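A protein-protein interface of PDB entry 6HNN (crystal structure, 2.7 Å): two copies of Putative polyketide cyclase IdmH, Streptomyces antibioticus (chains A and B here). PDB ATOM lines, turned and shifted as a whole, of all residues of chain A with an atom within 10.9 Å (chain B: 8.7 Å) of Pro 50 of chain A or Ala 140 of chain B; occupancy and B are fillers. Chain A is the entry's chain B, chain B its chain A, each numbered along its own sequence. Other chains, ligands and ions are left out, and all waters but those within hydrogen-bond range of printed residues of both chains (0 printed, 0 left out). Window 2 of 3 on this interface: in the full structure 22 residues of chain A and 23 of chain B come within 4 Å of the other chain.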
ATOM      1  N   ILE A  37      -7.479  -7.563  27.625  1.00  0.00           N
ATOM      2  CA  ILE A  37      -6.487  -6.938  26.741  1.00  0.00           C
ATOM      3  C   ILE A  37      -5.121  -7.622  26.891  1.00  0.00           C
ATOM      4  O   ILE A  37      -4.498  -7.558  27.952  1.00  0.00           O
ATOM      5  CB  ILE A  37      -6.329  -5.429  27.007  1.00  0.00           C
ATOM      6  CG1 ILE A  37      -7.692  -4.733  27.117  1.00  0.00           C
ATOM      7  CG2 ILE A  37      -5.505  -4.790  25.903  1.00  0.00           C
ATOM      8  CD1 ILE A  37      -8.570  -4.864  25.878  1.00  0.00           C
ATOM      9  N   HIS A  38      -4.686  -8.279  25.824  1.00  0.00           N
ATOM     10  CA  HIS A  38      -3.408  -8.960  25.762  1.00  0.00           C
ATOM     11  C   HIS A  38      -2.413  -8.006  25.102  1.00  0.00           C
ATOM     12  O   HIS A  38      -2.355  -7.892  23.891  1.00  0.00           O
ATOM     13  CB  HIS A  38      -3.533 -10.263  24.969  1.00  0.00           C
ATOM     14  CG  HIS A  38      -4.577 -11.191  25.483  1.00  0.00           C
ATOM     15  ND1 HIS A  38      -4.379 -12.000  26.582  1.00  0.00           N
ATOM     16  CD2 HIS A  38      -5.837 -11.447  25.044  1.00  0.00           C
ATOM     17  CE1 HIS A  38      -5.476 -12.713  26.801  1.00  0.00           C
ATOM     18  NE2 HIS A  38      -6.373 -12.398  25.877  1.00  0.00           N
ATOM     19  N   LEU A  39      -1.672  -7.289  25.917  1.00  0.00           N
ATOM     20  CA  LEU A  39      -0.620  -6.410  25.435  1.00  0.00           C
ATOM     21  C   LEU A  39       0.660  -7.216  25.374  1.00  0.00           C
ATOM     22  O   LEU A  39       0.825  -8.170  26.129  1.00  0.00           O
ATOM     23  CB  LEU A  39      -0.441  -5.234  26.393  1.00  0.00           C
ATOM     24  CG  LEU A  39      -1.634  -4.324  26.518  1.00  0.00           C
ATOM     25  CD1 LEU A  39      -1.340  -3.192  27.492  1.00  0.00           C
ATOM     26  CD2 LEU A  39      -2.041  -3.803  25.146  1.00  0.00           C
ATOM     27  N   PRO A  40       1.588  -6.813  24.518  1.00  0.00           N
ATOM     28  CA  PRO A  40       2.847  -7.546  24.449  1.00  0.00           C
ATOM     29  C   PRO A  40       3.669  -7.367  25.729  1.00  0.00           C
ATOM     30  O   PRO A  40       3.360  -6.490  26.548  1.00  0.00           O
ATOM     31  CB  PRO A  40       3.571  -6.901  23.253  1.00  0.00           C
ATOM     32  CG  PRO A  40       3.025  -5.522  23.167  1.00  0.00           C
ATOM     33  CD  PRO A  40       1.629  -5.559  23.726  1.00  0.00           C
ATOM     34  N   GLY A  41       4.712  -8.177  25.883  1.00  0.00           N
ATOM     35  CA  GLY A  41       5.554  -8.175  27.072  1.00  0.00           C
ATOM     36  C   GLY A  41       6.250  -6.857  27.369  1.00  0.00           C
ATOM     37  O   GLY A  41       6.515  -6.546  28.537  1.00  0.00           O
ATOM     38  N   THR A  42       6.538  -6.083  26.312  1.00  0.00           N
ATOM     39  CA  THR A  42       7.094  -4.744  26.467  1.00  0.00           C
ATOM     40  C   THR A  42       6.192  -3.836  27.310  1.00  0.00           C
ATOM     41  O   THR A  42       6.688  -2.944  27.975  1.00  0.00           O
ATOM     42  CB  THR A  42       7.313  -4.062  25.100  1.00  0.00           C
ATOM     43  OG1 THR A  42       6.107  -4.154  24.314  1.00  0.00           O
ATOM     44  CG2 THR A  42       8.478  -4.698  24.346  1.00  0.00           C
ATOM     45  N   ALA A  43       4.871  -4.070  27.292  1.00  0.00           N
ATOM     46  CA  ALA A  43       3.918  -3.294  28.086  1.00  0.00           C
ATOM     47  C   ALA A  43       3.767  -3.756  29.549  1.00  0.00           C
ATOM     48  O   ALA A  43       2.943  -3.208  30.312  1.00  0.00           O
ATOM     49  CB  ALA A  43       2.567  -3.291  27.410  1.00  0.00           C
ATOM     50  N   GLY A  44       4.533  -4.766  29.961  1.00  0.00           N
ATOM     51  CA  GLY A  44       4.447  -5.269  31.315  1.00  0.00           C
ATOM     52  C   GLY A  44       5.075  -4.319  32.302  1.00  0.00           C
ATOM     53  O   GLY A  44       5.816  -3.400  31.915  1.00  0.00           O
ATOM     54  N   ASP A  45       4.757  -4.532  33.575  1.00  0.00           N
ATOM     55  CA  ASP A  45       5.386  -3.829  34.683  1.00  0.00           C
ATOM     56  C   ASP A  45       5.472  -4.816  35.857  1.00  0.00           C
ATOM     57  O   ASP A  45       5.232  -6.008  35.668  1.00  0.00           O
ATOM     58  CB  ASP A  45       4.586  -2.555  35.050  1.00  0.00           C
ATOM     59  CG  ASP A  45       3.133  -2.809  35.354  1.00  0.00           C
ATOM     60  OD1 ASP A  45       2.782  -3.825  35.987  1.00  0.00           O
ATOM     61  OD2 ASP A  45       2.294  -1.965  34.963  1.00  0.00           O
ATOM     62  N   ALA A  46       5.815  -4.334  37.056  1.00  0.00           N
ATOM     63  CA  ALA A  46       5.903  -5.175  38.244  1.00  0.00           C
ATOM     64  C   ALA A  46       4.558  -5.797  38.629  1.00  0.00           C
ATOM     65  O   ALA A  46       4.460  -6.998  38.865  1.00  0.00           O
ATOM     66  CB  ALA A  46       6.465  -4.371  39.393  1.00  0.00           C
ATOM     67  N   GLU A  47       3.519  -4.982  38.687  1.00  0.00           N
ATOM     68  CA  GLU A  47       2.175  -5.465  39.034  1.00  0.00           C
ATOM     69  C   GLU A  47       1.575  -6.441  37.978  1.00  0.00           C
ATOM     70  O   GLU A  47       0.756  -7.285  38.328  1.00  0.00           O
ATOM     71  CB  GLU A  47       1.239  -4.268  39.272  1.00  0.00           C
ATOM     72  N   HIS A  48       1.996  -6.322  36.712  1.00  0.00           N
ATOM     73  CA  HIS A  48       1.429  -7.093  35.586  1.00  0.00           C
ATOM     74  C   HIS A  48       2.520  -7.696  34.699  1.00  0.00           C
ATOM     75  O   HIS A  48       2.906  -7.090  33.699  1.00  0.00           O
ATOM     76  CB  HIS A  48       0.530  -6.200  34.732  1.00  0.00           C
ATOM     77  CG  HIS A  48      -0.569  -5.551  35.500  1.00  0.00           C
ATOM     78  ND1 HIS A  48      -0.382  -4.392  36.232  1.00  0.00           N
ATOM     79  CD2 HIS A  48      -1.865  -5.895  35.648  1.00  0.00           C
ATOM     80  CE1 HIS A  48      -1.524  -4.064  36.814  1.00  0.00           C
ATOM     81  NE2 HIS A  48      -2.441  -4.957  36.471  1.00  0.00           N
ATOM     82  N   PRO A  49       3.026  -8.893  35.052  1.00  0.00           N
ATOM     83  CA  PRO A  49       4.083  -9.546  34.277  1.00  0.00           C
ATOM     84  C   PRO A  49       3.774  -9.710  32.783  1.00  0.00           C
ATOM     85  O   PRO A  49       2.606  -9.805  32.413  1.00  0.00           O
ATOM     86  CB  PRO A  49       4.162 -10.952  34.908  1.00  0.00           C
ATOM     87  CG  PRO A  49       3.651 -10.790  36.290  1.00  0.00           C
ATOM     88  CD  PRO A  49       2.687  -9.650  36.271  1.00  0.00           C
ATOM     89  N   PRO A  50       4.817  -9.758  31.932  1.00  0.00           N
ATOM     90  CA  PRO A  50       4.654 -10.082  30.523  1.00  0.00           C
ATOM     91  C   PRO A  50       3.730 -11.275  30.287  1.00  0.00           C
ATOM     92  O   PRO A  50       3.891 -12.302  30.905  1.00  0.00           O
ATOM     93  CB  PRO A  50       6.073 -10.407  30.085  1.00  0.00           C
ATOM     94  CG  PRO A  50       6.919  -9.517  30.932  1.00  0.00           C
ATOM     95  CD  PRO A  50       6.228  -9.452  32.247  1.00  0.00           C
ATOM     96  N   GLY A  51       2.748 -11.104  29.414  1.00  0.00           N
ATOM     97  CA  GLY A  51       1.782 -12.126  29.081  1.00  0.00           C
ATOM     98  C   GLY A  51       0.556 -12.226  29.964  1.00  0.00           C
ATOM     99  O   GLY A  51      -0.320 -13.036  29.683  1.00  0.00           O
ATOM    100  N   THR A  52       0.468 -11.455  31.042  1.00  0.00           N
ATOM    101  CA  THR A  52      -0.755 -11.418  31.855  1.00  0.00           C
ATOM    102  C   THR A  52      -1.676 -10.371  31.259  1.00  0.00           C
ATOM    103  O   THR A  52      -1.225  -9.295  30.909  1.00  0.00           O
ATOM    104  CB  THR A  52      -0.492 -11.122  33.353  1.00  0.00           C
ATOM    105  OG1 THR A  52      -0.048  -9.784  33.516  1.00  0.00           O
ATOM    106  CG2 THR A  52       0.548 -12.083  33.922  1.00  0.00           C
ATOM    107  N   PRO A  53      -2.976 -10.680  31.157  1.00  0.00           N
ATOM    108  CA  PRO A  53      -3.889  -9.721  30.515  1.00  0.00           C
ATOM    109  C   PRO A  53      -4.211  -8.533  31.413  1.00  0.00           C
ATOM    110  O   PRO A  53      -3.889  -8.531  32.613  1.00  0.00           O
ATOM    111  CB  PRO A  53      -5.144 -10.550  30.278  1.00  0.00           C
ATOM    112  CG  PRO A  53      -5.114 -11.567  31.380  1.00  0.00           C
ATOM    113  CD  PRO A  53      -3.675 -11.887  31.652  1.00  0.00           C
ATOM    114  N   ARG A  54      -4.835  -7.524  30.818  1.00  0.00           N
ATOM    115  CA  ARG A  54      -5.294  -6.346  31.534  1.00  0.00           C
ATOM    116  C   ARG A  54      -6.717  -6.029  31.143  1.00  0.00           C
ATOM    117  O   ARG A  54      -7.205  -6.517  30.123  1.00  0.00           O
ATOM    118  CB  ARG A  54      -4.410  -5.158  31.198  1.00  0.00           C
ATOM    119  CG  ARG A  54      -2.977  -5.265  31.696  1.00  0.00           C
ATOM    120  CD  ARG A  54      -2.157  -4.242  30.919  1.00  0.00           C
ATOM    121  NE  ARG A  54      -0.887  -3.870  31.544  1.00  0.00           N
ATOM    122  CZ  ARG A  54      -0.770  -3.135  32.651  1.00  0.00           C
ATOM    123  NH1 ARG A  54      -1.833  -2.733  33.364  1.00  0.00           N
ATOM    124  NH2 ARG A  54       0.452  -2.835  33.073  1.00  0.00           N
ATOM    125  N   THR A 131      -2.476  -7.362  20.693  1.00  0.00           N
ATOM    126  CA  THR A 131      -1.662  -6.422  19.923  1.00  0.00           C
ATOM    127  C   THR A 131      -0.172  -6.678  20.135  1.00  0.00           C
ATOM    128  O   THR A 131       0.228  -7.055  21.218  1.00  0.00           O
ATOM    129  CB  THR A 131      -2.052  -4.949  20.249  1.00  0.00           C
ATOM    130  OG1 THR A 131      -1.182  -4.045  19.560  1.00  0.00           O
ATOM    131  CG2 THR A 131      -2.003  -4.645  21.719  1.00  0.00           C
ATOM    132  N   PHE B 101      20.838 -21.338  24.572  1.00  0.00           N
ATOM    133  CA  PHE B 101      20.770 -20.141  23.789  1.00  0.00           C
ATOM    134  C   PHE B 101      20.842 -18.910  24.690  1.00  0.00           C
ATOM    135  O   PHE B 101      20.536 -18.955  25.913  1.00  0.00           O
ATOM    136  CB  PHE B 101      19.509 -20.187  22.970  1.00  0.00           C
ATOM    137  CG  PHE B 101      18.307 -19.726  23.679  1.00  0.00           C
ATOM    138  CD1 PHE B 101      17.597 -20.532  24.548  1.00  0.00           C
ATOM    139  CD2 PHE B 101      17.802 -18.479  23.373  1.00  0.00           C
ATOM    140  CE1 PHE B 101      16.481 -20.037  25.201  1.00  0.00           C
ATOM    141  CE2 PHE B 101      16.616 -18.028  23.943  1.00  0.00           C
ATOM    142  CZ  PHE B 101      16.014 -18.775  24.921  1.00  0.00           C
ATOM    143  N   ARG B 109      12.176 -25.838  30.673  1.00  0.00           N
ATOM    144  CA  ARG B 109      10.980 -25.002  30.937  1.00  0.00           C
ATOM    145  C   ARG B 109      10.144 -24.727  29.689  1.00  0.00           C
ATOM    146  O   ARG B 109      10.700 -24.577  28.620  1.00  0.00           O
ATOM    147  CB  ARG B 109      11.371 -23.685  31.603  1.00  0.00           C
ATOM    148  CG  ARG B 109      11.943 -23.794  32.996  1.00  0.00           C
ATOM    149  CD  ARG B 109      12.408 -22.439  33.455  1.00  0.00           C
ATOM    150  NE  ARG B 109      13.047 -22.500  34.753  1.00  0.00           N
ATOM    151  CZ  ARG B 109      13.580 -21.455  35.384  1.00  0.00           C
ATOM    152  NH1 ARG B 109      13.563 -20.230  34.849  1.00  0.00           N
ATOM    153  NH2 ARG B 109      14.144 -21.631  36.570  1.00  0.00           N
ATOM    154  N   PRO B 110       8.825 -24.678  29.831  1.00  0.00           N
ATOM    155  CA  PRO B 110       7.982 -24.502  28.599  1.00  0.00           C
ATOM    156  C   PRO B 110       7.798 -22.994  28.316  1.00  0.00           C
ATOM    157  O   PRO B 110       8.014 -22.137  29.201  1.00  0.00           O
ATOM    158  CB  PRO B 110       6.637 -25.069  29.038  1.00  0.00           C
ATOM    159  CG  PRO B 110       6.598 -24.753  30.546  1.00  0.00           C
ATOM    160  CD  PRO B 110       8.026 -24.893  31.063  1.00  0.00           C
ATOM    161  N   PHE B 111       7.392 -22.672  27.098  1.00  0.00           N
ATOM    162  CA  PHE B 111       6.902 -21.331  26.778  1.00  0.00           C
ATOM    163  C   PHE B 111       5.701 -21.385  25.861  1.00  0.00           C
ATOM    164  O   PHE B 111       5.535 -22.335  25.090  1.00  0.00           O
ATOM    165  CB  PHE B 111       8.004 -20.459  26.150  1.00  0.00           C
ATOM    166  CG  PHE B 111       8.503 -20.979  24.842  1.00  0.00           C
ATOM    167  CD1 PHE B 111       7.867 -20.646  23.687  1.00  0.00           C
ATOM    168  CD2 PHE B 111       9.637 -21.796  24.787  1.00  0.00           C
ATOM    169  CE1 PHE B 111       8.338 -21.112  22.464  1.00  0.00           C
ATOM    170  CE2 PHE B 111      10.112 -22.273  23.614  1.00  0.00           C
ATOM    171  CZ  PHE B 111       9.471 -21.925  22.430  1.00  0.00           C
ATOM    172  N   GLU B 112       4.909 -20.322  25.902  1.00  0.00           N
ATOM    173  CA  GLU B 112       3.670 -20.197  25.152  1.00  0.00           C
ATOM    174  C   GLU B 112       3.594 -18.728  24.743  1.00  0.00           C
ATOM    175  O   GLU B 112       3.448 -17.871  25.594  1.00  0.00           O
ATOM    176  CB  GLU B 112       2.509 -20.582  26.059  1.00  0.00           C
ATOM    177  CG  GLU B 112       1.152 -20.681  25.375  1.00  0.00           C
ATOM    178  CD  GLU B 112       0.104 -21.398  26.186  1.00  0.00           C
ATOM    179  OE1 GLU B 112       0.374 -22.579  26.503  1.00  0.00           O
ATOM    180  OE2 GLU B 112      -0.993 -20.826  26.400  1.00  0.00           O
ATOM    181  N   ASP B 134       5.410 -12.371  20.233  1.00  0.00           N
ATOM    182  CA  ASP B 134       5.630 -11.736  21.511  1.00  0.00           C
ATOM    183  C   ASP B 134       6.879 -12.297  22.185  1.00  0.00           C
ATOM    184  O   ASP B 134       6.814 -13.077  23.152  1.00  0.00           O
ATOM    185  CB  ASP B 134       4.395 -11.894  22.384  1.00  0.00           C
ATOM    186  CG  ASP B 134       4.402 -10.944  23.583  1.00  0.00           C
ATOM    187  OD1 ASP B 134       5.417 -10.205  23.773  1.00  0.00           O
ATOM    188  OD2 ASP B 134       3.391 -10.949  24.324  1.00  0.00           O
ATOM    189  N   ASN B 135       8.036 -11.895  21.681  1.00  0.00           N
ATOM    190  CA  ASN B 135       9.309 -12.495  22.083  1.00  0.00           C
ATOM    191  C   ASN B 135       9.666 -12.213  23.539  1.00  0.00           C
ATOM    192  O   ASN B 135      10.279 -13.048  24.185  1.00  0.00           O
ATOM    193  CB  ASN B 135      10.438 -12.008  21.174  1.00  0.00           C
ATOM    194  CG  ASN B 135      10.546 -12.837  19.910  1.00  0.00           C
ATOM    195  OD1 ASN B 135      10.983 -14.006  19.937  1.00  0.00           O
ATOM    196  ND2 ASN B 135      10.099 -12.250  18.799  1.00  0.00           N
ATOM    197  N   VAL B 136       9.300 -11.029  24.039  1.00  0.00           N
ATOM    198  CA  VAL B 136       9.643 -10.628  25.388  1.00  0.00           C
ATOM    199  C   VAL B 136       8.907 -11.485  26.406  1.00  0.00           C
ATOM    200  O   VAL B 136       9.479 -11.859  27.431  1.00  0.00           O
ATOM    201  CB  VAL B 136       9.334  -9.131  25.618  1.00  0.00           C
ATOM    202  CG1 VAL B 136       9.465  -8.730  27.103  1.00  0.00           C
ATOM    203  CG2 VAL B 136      10.261  -8.288  24.742  1.00  0.00           C
ATOM    204  N   THR B 137       7.643 -11.796  26.113  1.00  0.00           N
ATOM    205  CA  THR B 137       6.871 -12.701  26.940  1.00  0.00           C
ATOM    206  C   THR B 137       7.471 -14.099  26.967  1.00  0.00           C
ATOM    207  O   THR B 137       7.490 -14.726  28.020  1.00  0.00           O
ATOM    208  CB  THR B 137       5.409 -12.742  26.475  1.00  0.00           C
ATOM    209  OG1 THR B 137       4.819 -11.451  26.667  1.00  0.00           O
ATOM    210  CG2 THR B 137       4.596 -13.809  27.269  1.00  0.00           C
ATOM    211  N   MET B 138       7.959 -14.591  25.829  1.00  0.00           N
ATOM    212  CA  MET B 138       8.647 -15.884  25.808  1.00  0.00           C
ATOM    213  C   MET B 138       9.845 -15.873  26.740  1.00  0.00           C
ATOM    214  O   MET B 138      10.006 -16.787  27.540  1.00  0.00           O
ATOM    215  CB  MET B 138       9.093 -16.271  24.408  1.00  0.00           C
ATOM    216  CG  MET B 138      10.082 -17.440  24.407  1.00  0.00           C
ATOM    217  SD  MET B 138      10.556 -17.932  22.758  1.00  0.00           S
ATOM    218  CE  MET B 138      11.712 -16.587  22.379  1.00  0.00           C
ATOM    219  N   LEU B 139      10.686 -14.852  26.634  1.00  0.00           N
ATOM    220  CA  LEU B 139      11.851 -14.742  27.503  1.00  0.00           C
ATOM    221  C   LEU B 139      11.456 -14.644  28.981  1.00  0.00           C
ATOM    222  O   LEU B 139      12.093 -15.264  29.831  1.00  0.00           O
ATOM    223  CB  LEU B 139      12.731 -13.551  27.095  1.00  0.00           C
ATOM    224  CG  LEU B 139      13.366 -13.665  25.682  1.00  0.00           C
ATOM    225  CD1 LEU B 139      14.239 -12.471  25.368  1.00  0.00           C
ATOM    226  CD2 LEU B 139      14.179 -14.954  25.512  1.00  0.00           C
ATOM    227  N   ALA B 140      10.406 -13.892  29.284  1.00  0.00           N
ATOM    228  CA  ALA B 140       9.907 -13.808  30.656  1.00  0.00           C
ATOM    229  C   ALA B 140       9.449 -15.172  31.154  1.00  0.00           C
ATOM    230  O   ALA B 140       9.820 -15.582  32.240  1.00  0.00           O
ATOM    231  CB  ALA B 140       8.769 -12.804  30.759  1.00  0.00           C
ATOM    232  N   GLN B 141       8.665 -15.889  30.361  1.00  0.00           N
ATOM    233  CA  GLN B 141       8.267 -17.256  30.708  1.00  0.00           C
ATOM    234  C   GLN B 141       9.445 -18.181  30.970  1.00  0.00           C
ATOM    235  O   GLN B 141       9.389 -18.973  31.913  1.00  0.00           O
ATOM    236  CB  GLN B 141       7.363 -17.851  29.639  1.00  0.00           C
ATOM    237  CG  GLN B 141       5.971 -17.262  29.638  1.00  0.00           C
ATOM    238  CD  GLN B 141       5.177 -17.568  28.384  1.00  0.00           C
ATOM    239  OE1 GLN B 141       5.641 -18.209  27.467  1.00  0.00           O
ATOM    240  NE2 GLN B 141       3.960 -17.067  28.332  1.00  0.00           N
ATOM    241  N   LEU B 142      10.518 -18.080  30.186  1.00  0.00           N
ATOM    242  CA  LEU B 142      11.686 -18.934  30.403  1.00  0.00           C
ATOM    243  C   LEU B 142      12.497 -18.591  31.651  1.00  0.00           C
ATOM    244  O   LEU B 142      13.208 -19.468  32.134  1.00  0.00           O
ATOM    245  CB  LEU B 142      12.590 -18.964  29.157  1.00  0.00           C
ATOM    246  CG  LEU B 142      11.979 -19.579  27.875  1.00  0.00           C
ATOM    247  CD1 LEU B 142      12.939 -19.558  26.711  1.00  0.00           C
ATOM    248  CD2 LEU B 142      11.536 -21.021  28.050  1.00  0.00           C
ATOM    249  N   GLY B 143      12.288 -17.406  32.254  1.00  0.00           N
ATOM    250  CA  GLY B 143      12.967 -17.009  33.494  1.00  0.00           C
ATOM    251  C   GLY B 143      12.087 -16.961  34.727  1.00  0.00           C
ATOM    252  O   GLY B 143      12.111 -15.968  35.451  1.00  0.00           O
ATOM    253  N   VAL B 144      11.192 -17.952  34.854  1.00  0.00           N
ATOM    254  CA  VAL B 144      10.127 -17.952  35.885  1.00  0.00           C
ATOM    255  C   VAL B 144       9.333 -19.264  35.865  1.00  0.00           C
ATOM    256  O   VAL B 144       8.239 -19.325  35.303  1.00  0.00           O
ATOM    257  CB  VAL B 144       9.151 -16.731  35.758  1.00  0.00           C
ATOM    258  N   LYS B 145       9.911 -20.317  36.452  1.00  0.00           N
ATOM    259  CA  LYS B 145       9.157 -21.529  36.887  1.00  0.00           C
ATOM    260  C   LYS B 145       9.045 -21.582  38.442  1.00  0.00           C
ATOM    261  O   LYS B 145      10.069 -21.665  39.155  1.00  0.00           O
ATOM    262  CB  LYS B 145       9.778 -22.821  36.336  1.00  0.00           C
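The backbone NH of Gly 41 of chain A lies within hydrogen-bond range of the side-chain carboxylate of Asp 134 of chain B (3.0 Å). The side-chain hydroxyl (OG1) of Thr 137 of chain B sits at hydrogen-bond distance from the backbone NH (N) of Gly 41 of chain A. The backbone NH (N) of Gly 51 of chain A sits at hydrogen-bond distance from the side-chain hydroxyl (OG1) of Thr 137 of chain B.
OG1 of Thr 137 of chain B sits at hydrogen-bond distance from OD2 of Asp 134 of chain B, 2.8 Å away.
Asp 134 of chain B touches Pro 40 of chain A. Val 136 of chain B touches Gly 41 of chain A. C of Pro 50 of chain A touches OG1 of Thr 137 of chain B, 3.8 Å away. Pro 50 of chain A touches Ala 140 of chain B (CB to CB, 3.7 Å).
Of the printed residues of chain B, Pro 40 of chain A touches Asp 134. Of chain B, only Thr 137 (3.8 Å) and Ala 140 (3.7 Å) come within 4 Å of Pro 50 of chain A. Gly 51 of chain A touches just one residue of chain B: Thr 137 (3.5 Å). Of the printed residues of chain A, Asp 134 of chain B touches Pro 40 and Gly 41. Printed residues of chain A within 4 Å of Val 136 of chain B: Gly 41 (3.7 Å). No residue of chain A comes within 4 Å of Leu 139 of chain B. Ala 140 of chain B touches just one residue of chain A: Pro 50 (3.7 Å). Gly 143 of chain B touches none of the printed residues of chain A. The nearest residue of chain B that does not touch Pro 50 of chain A is Val 136 of chain B (4.6 Å).
Of the 19 printed residues of chain A, 4 touch a printed residue of chain B. Printed residues of chain A that touch a printed residue of chain B: Pro 40, Gly 41, Pro 50 and Gly 51. Hydrophobic or aromatic side chains of chain A that line the printed part of chain B: Pro 40 and Pro 50. Among the printed residues, 7 pairs touch across the chains. Among the printed residues, no Asp or Glu carboxylate lies within 4 Å of a Lys or Arg side-chain nitrogen of the other chain.
No position is printed for both chains.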
